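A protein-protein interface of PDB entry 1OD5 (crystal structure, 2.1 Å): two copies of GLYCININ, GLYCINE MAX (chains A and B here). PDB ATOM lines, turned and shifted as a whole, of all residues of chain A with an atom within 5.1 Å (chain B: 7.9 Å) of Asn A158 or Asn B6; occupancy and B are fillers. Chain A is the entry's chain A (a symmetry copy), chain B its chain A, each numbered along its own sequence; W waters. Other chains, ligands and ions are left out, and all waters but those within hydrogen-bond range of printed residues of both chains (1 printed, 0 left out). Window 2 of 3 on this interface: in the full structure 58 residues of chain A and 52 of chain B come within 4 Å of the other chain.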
ATOM      1  N   TYR A  64     -24.883  35.331  15.990  1.00  0.00           N
ATOM      2  CA  TYR A  64     -23.438  35.485  16.133  1.00  0.00           C
ATOM      3  C   TYR A  64     -23.127  36.964  16.222  1.00  0.00           C
ATOM      4  O   TYR A  64     -23.968  37.779  15.840  1.00  0.00           O
ATOM      5  CB  TYR A  64     -22.694  34.874  14.914  1.00  0.00           C
ATOM      6  CG  TYR A  64     -23.350  35.146  13.558  1.00  0.00           C
ATOM      7  CD1 TYR A  64     -24.171  34.164  12.979  1.00  0.00           C
ATOM      8  CD2 TYR A  64     -23.195  36.384  12.936  1.00  0.00           C
ATOM      9  CE1 TYR A  64     -24.846  34.419  11.796  1.00  0.00           C
ATOM     10  CE2 TYR A  64     -23.869  36.648  11.755  1.00  0.00           C
ATOM     11  CZ  TYR A  64     -24.690  35.665  11.213  1.00  0.00           C
ATOM     12  OH  TYR A  64     -25.418  35.988  10.103  1.00  0.00           O
ATOM     13  N   THR A 148     -19.685  33.841  11.880  1.00  0.00           N
ATOM     14  CA  THR A 148     -20.519  32.661  11.982  1.00  0.00           C
ATOM     15  C   THR A 148     -19.862  31.519  12.703  1.00  0.00           C
ATOM     16  O   THR A 148     -20.569  30.695  13.269  1.00  0.00           O
ATOM     17  CB  THR A 148     -20.944  32.269  10.567  1.00  0.00           C
ATOM     18  OG1 THR A 148     -19.759  32.133   9.825  1.00  0.00           O
ATOM     19  CG2 THR A 148     -21.796  33.322   9.875  1.00  0.00           C
ATOM     20  N   ASP A 156     -25.438  26.899  13.251  1.00  0.00           N
ATOM     21  CA  ASP A 156     -24.422  26.320  12.359  1.00  0.00           C
ATOM     22  C   ASP A 156     -23.831  27.459  11.584  1.00  0.00           C
ATOM     23  O   ASP A 156     -24.422  28.539  11.612  1.00  0.00           O
ATOM     24  CB  ASP A 156     -24.990  25.293  11.345  1.00  0.00           C
ATOM     25  CG  ASP A 156     -26.226  25.748  10.608  1.00  0.00           C
ATOM     26  OD1 ASP A 156     -27.197  25.010  10.621  1.00  0.00           O
ATOM     27  OD2 ASP A 156     -26.248  26.826  10.029  1.00  0.00           O
ATOM     28  N   GLN A 157     -22.754  27.226  10.832  1.00  0.00           N
ATOM     29  CA  GLN A 157     -22.114  28.268  10.042  1.00  0.00           C
ATOM     30  C   GLN A 157     -22.942  28.986   9.008  1.00  0.00           C
ATOM     31  O   GLN A 157     -22.382  29.825   8.309  1.00  0.00           O
ATOM     32  CB  GLN A 157     -20.905  27.762   9.267  1.00  0.00           C
ATOM     33  CG  GLN A 157     -19.560  28.334   9.713  1.00  0.00           C
ATOM     34  CD  GLN A 157     -19.085  27.649  10.987  1.00  0.00           C
ATOM     35  OE1 GLN A 157     -19.813  27.526  11.978  1.00  0.00           O
ATOM     36  NE2 GLN A 157     -17.851  27.153  10.969  1.00  0.00           N
ATOM     37  N   ASN A 158     -24.223  28.730   8.838  1.00  0.00           N
ATOM     38  CA  ASN A 158     -24.941  29.446   7.825  1.00  0.00           C
ATOM     39  C   ASN A 158     -25.355  30.791   8.401  1.00  0.00           C
ATOM     40  O   ASN A 158     -25.903  30.844   9.501  1.00  0.00           O
ATOM     41  CB  ASN A 158     -26.124  28.554   7.376  1.00  0.00           C
ATOM     42  CG  ASN A 158     -25.653  27.221   6.702  1.00  0.00           C
ATOM     43  OD1 ASN A 158     -25.681  26.103   7.269  1.00  0.00           O
ATOM     44  ND2 ASN A 158     -25.074  27.281   5.497  1.00  0.00           N
ATOM     45  N   PRO A 159     -25.032  31.917   7.745  1.00  0.00           N
ATOM     46  CA  PRO A 159     -25.561  33.216   8.082  1.00  0.00           C
ATOM     47  C   PRO A 159     -27.065  33.250   8.101  1.00  0.00           C
ATOM     48  O   PRO A 159     -27.754  32.675   7.260  1.00  0.00           O
ATOM     49  CB  PRO A 159     -24.945  34.145   7.078  1.00  0.00           C
ATOM     50  CG  PRO A 159     -24.338  33.270   6.017  1.00  0.00           C
ATOM     51  CD  PRO A 159     -23.929  32.068   6.797  1.00  0.00           C
ATOM     52  N   ARG A 160     -27.543  33.734   9.238  1.00  0.00           N
ATOM     53  CA  ARG A 160     -28.957  33.893   9.483  1.00  0.00           C
ATOM     54  C   ARG A 160     -29.196  35.329   9.909  1.00  0.00           C
ATOM     55  O   ARG A 160     -28.346  35.944  10.540  1.00  0.00           O
ATOM     56  CB  ARG A 160     -29.411  32.992  10.564  1.00  0.00           C
ATOM     57  CG  ARG A 160     -29.350  31.581  10.068  1.00  0.00           C
ATOM     58  CD  ARG A 160     -29.921  30.756  11.149  1.00  0.00           C
ATOM     59  NE  ARG A 160     -30.155  29.395  10.742  1.00  0.00           N
ATOM     60  CZ  ARG A 160     -29.188  28.484  10.727  1.00  0.00           C
ATOM     61  NH1 ARG A 160     -29.505  27.252  10.355  1.00  0.00           N
ATOM     62  NH2 ARG A 160     -27.924  28.784  11.037  1.00  0.00           N
ATOM     63  N   THR A 175     -26.289  29.887   1.337  1.00  0.00           N
ATOM     64  CA  THR A 175     -26.573  29.103   2.530  1.00  0.00           C
ATOM     65  C   THR A 175     -28.069  28.995   2.742  1.00  0.00           C
ATOM     66  O   THR A 175     -28.700  29.444   3.718  1.00  0.00           O
ATOM     67  CB  THR A 175     -25.881  29.783   3.719  1.00  0.00           C
ATOM     68  OG1 THR A 175     -26.440  31.084   3.801  1.00  0.00           O
ATOM     69  CG2 THR A 175     -24.353  29.861   3.570  1.00  0.00           C
ATOM     70  N   ASN B   6     -25.110  22.827   8.298  1.00  0.00           N
ATOM     71  CA  ASN B   6     -26.422  22.444   7.818  1.00  0.00           C
ATOM     72  C   ASN B   6     -27.320  21.917   8.922  1.00  0.00           C
ATOM     73  O   ASN B   6     -28.539  21.974   8.737  1.00  0.00           O
ATOM     74  CB  ASN B   6     -26.352  21.324   6.735  1.00  0.00           C
ATOM     75  CG  ASN B   6     -26.103  19.897   7.276  1.00  0.00           C
ATOM     76  OD1 ASN B   6     -24.970  19.416   7.431  1.00  0.00           O
ATOM     77  ND2 ASN B   6     -27.188  19.188   7.613  1.00  0.00           N
ATOM     78  N   GLU B   7     -26.792  21.412  10.053  1.00  0.00           N
ATOM     79  CA  GLU B   7     -27.632  20.828  11.099  1.00  0.00           C
ATOM     80  C   GLU B   7     -28.787  21.551  11.705  1.00  0.00           C
ATOM     81  O   GLU B   7     -29.657  20.873  12.230  1.00  0.00           O
ATOM     82  CB  GLU B   7     -26.765  20.377  12.229  1.00  0.00           C
ATOM     83  CG  GLU B   7     -26.329  18.972  11.897  1.00  0.00           C
ATOM     84  CD  GLU B   7     -25.150  18.512  12.729  1.00  0.00           C
ATOM     85  OE1 GLU B   7     -25.252  18.545  13.955  1.00  0.00           O
ATOM     86  OE2 GLU B   7     -24.129  18.134  12.143  1.00  0.00           O
ATOM     87  N   CYS B   8     -28.843  22.873  11.620  1.00  0.00           N
ATOM     88  CA  CYS B   8     -29.964  23.599  12.181  1.00  0.00           C
ATOM     89  C   CYS B   8     -30.790  24.302  11.116  1.00  0.00           C
ATOM     90  O   CYS B   8     -31.688  25.117  11.347  1.00  0.00           O
ATOM     91  CB  CYS B   8     -29.421  24.572  13.237  1.00  0.00           C
ATOM     92  SG  CYS B   8     -28.963  23.668  14.746  1.00  0.00           S
ATOM     93  N   GLN B   9     -30.502  23.908   9.883  1.00  0.00           N
ATOM     94  CA  GLN B   9     -31.209  24.445   8.738  1.00  0.00           C
ATOM     95  C   GLN B   9     -32.287  23.369   8.561  1.00  0.00           C
ATOM     96  O   GLN B   9     -32.141  22.453   7.750  1.00  0.00           O
ATOM     97  CB  GLN B   9     -30.172  24.524   7.648  1.00  0.00           C
ATOM     98  CG  GLN B   9     -30.593  25.429   6.546  1.00  0.00           C
ATOM     99  CD  GLN B   9     -29.411  26.070   5.835  1.00  0.00           C
ATOM    100  OE1 GLN B   9     -28.308  25.518   5.661  1.00  0.00           O
ATOM    101  NE2 GLN B   9     -29.682  27.313   5.426  1.00  0.00           N
ATOM    102  N   LEU B  10     -33.324  23.429   9.422  1.00  0.00           N
ATOM    103  CA  LEU B  10     -34.447  22.484   9.480  1.00  0.00           C
ATOM    104  C   LEU B  10     -35.755  23.146   9.132  1.00  0.00           C
ATOM    105  O   LEU B  10     -36.208  23.959   9.932  1.00  0.00           O
ATOM    106  CB  LEU B  10     -34.637  21.926  10.868  1.00  0.00           C
ATOM    107  CG  LEU B  10     -33.466  21.288  11.564  1.00  0.00           C
ATOM    108  CD1 LEU B  10     -33.790  21.199  13.047  1.00  0.00           C
ATOM    109  CD2 LEU B  10     -33.157  19.937  10.935  1.00  0.00           C
ATOM    110  N   PRO B  37     -33.019  14.798  13.598  1.00  0.00           N
ATOM    111  CA  PRO B  37     -32.437  16.047  13.140  1.00  0.00           C
ATOM    112  C   PRO B  37     -32.518  17.203  14.156  1.00  0.00           C
ATOM    113  O   PRO B  37     -31.584  17.985  14.276  1.00  0.00           O
ATOM    114  CB  PRO B  37     -33.197  16.338  11.864  1.00  0.00           C
ATOM    115  CG  PRO B  37     -33.637  14.998  11.385  1.00  0.00           C
ATOM    116  CD  PRO B  37     -34.088  14.406  12.678  1.00  0.00           C
ATOM    117  N   GLN B  40     -30.103  16.649  16.906  1.00  0.00           N
ATOM    118  CA  GLN B  40     -28.752  16.864  16.418  1.00  0.00           C
ATOM    119  C   GLN B  40     -28.381  18.321  16.255  1.00  0.00           C
ATOM    120  O   GLN B  40     -27.220  18.713  16.284  1.00  0.00           O
ATOM    121  CB  GLN B  40     -28.557  16.190  15.091  1.00  0.00           C
ATOM    122  CG  GLN B  40     -28.394  14.695  15.258  1.00  0.00           C
ATOM    123  CD  GLN B  40     -27.993  14.130  13.913  1.00  0.00           C
ATOM    124  OE1 GLN B  40     -26.807  14.164  13.580  1.00  0.00           O
ATOM    125  NE2 GLN B  40     -28.933  13.645  13.092  1.00  0.00           N
ATOM    126  N   CYS B  41     -29.384  19.148  16.051  1.00  0.00           N
ATOM    127  CA  CYS B  41     -29.190  20.579  15.912  1.00  0.00           C
ATOM    128  C   CYS B  41     -28.799  21.148  17.276  1.00  0.00           C
ATOM    129  O   CYS B  41     -27.832  21.889  17.373  1.00  0.00           O
ATOM    130  CB  CYS B  41     -30.487  21.127  15.414  1.00  0.00           C
ATOM    131  SG  CYS B  41     -30.657  22.906  15.440  1.00  0.00           S
ATOM    132  N   CYS B 405     -35.841  31.929  10.464  1.00  0.00           N
ATOM    133  CA  CYS B 405     -35.485  33.209   9.904  1.00  0.00           C
ATOM    134  C   CYS B 405     -36.118  33.623   8.607  1.00  0.00           C
ATOM    135  O   CYS B 405     -35.916  34.749   8.155  1.00  0.00           O
ATOM    136  CB  CYS B 405     -33.977  33.285   9.759  1.00  0.00           C
ATOM    137  SG  CYS B 405     -33.227  31.894   8.891  1.00  0.00           S
HETATM  138  O   HOH W   1     -32.472  27.809   9.518  1.00  0.00           O
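Water W1 lies within hydrogen-bond range of NE of Arg A160 (3.1 Å) and O of Cys B8 (3.3 Å).
O of Cys B8 is in hydrogen-bond range of NH1 of Arg A160, 3.2 Å away.
OE1 of Gln B9 lies close to OD1 of Asn A158 (3.1 Å).
N of Asn B6 lies within hydrogen-bond range of OD1 of Asn A158, at 3.5 Å.
The backbone carbonyl oxygen of Thr A175 lies within hydrogen-bond range of the side-chain amide nitrogen of Gln B9, 2.9 Å away.
OD1 of Asp A156 lies within hydrogen-bond range of N of Cys B8, 2.9 Å away.
Asn A158 touches just these residues of chain B: Asn B6 and Gln B9.
Printed residues of chain A within 4 Å of Asn B6: Asp A156 (3.5 Å) and Asn A158 (3.5 Å).
No residue of chain B comes within 4 Å of Pro A159.
Printed residues of chain A within 4 Å of Glu B7: Asp A156.
Of the printed residues of chain B, Arg A160 touches Cys B8 (3.2 Å) and Gln B9 (3.5 Å).
Of the printed residues of chain B, Thr A175 touches Gln B9.
The nearest residue of chain B that does not touch Asn A158 is Glu B7 (5.6 Å).
The nearest printed residue of chain A that does not touch Asn B6 is Gln A157 (5.6 Å).
OH of Tyr A64 is in hydrogen-bond range of O of Arg A160, 3.0 Å away.
The side-chain amide oxygen (OD1) of Asn A158 lies close to the side-chain carboxylate (OD2) of Asp A156 (2.9 Å).
The guanidinium group (NH2) of Arg A160 is in hydrogen-bond range of the backbone carbonyl oxygen (O) of Asn A158.
SG of Cys B41 forms a disulfide with SG of Cys B8, at 2.0 Å.
NH2 of Arg A160 lies within salt-bridge range of OD2 of Asp A156.
Printed residues of chain B that touch a printed residue of chain A: Asn B6, Glu B7, Cys B8 and Gln B9.
Along chain B the printed residues that touch a printed residue of chain A span positions 6 to 9.
Along chain A the printed residues that touch a printed residue of chain B span positions 156 to 175.
No position is printed for both chains.
Of the 9 pairs that touch across the chains among the printed residues, none has its exchanged pair printed and touching as well.
Among the printed residues, merely in contact across the chains: Arg A160 with Gln B9, Asp A156 with Asn B6, Asp A156 with Gln B9 and Asp A156 with Glu B7.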
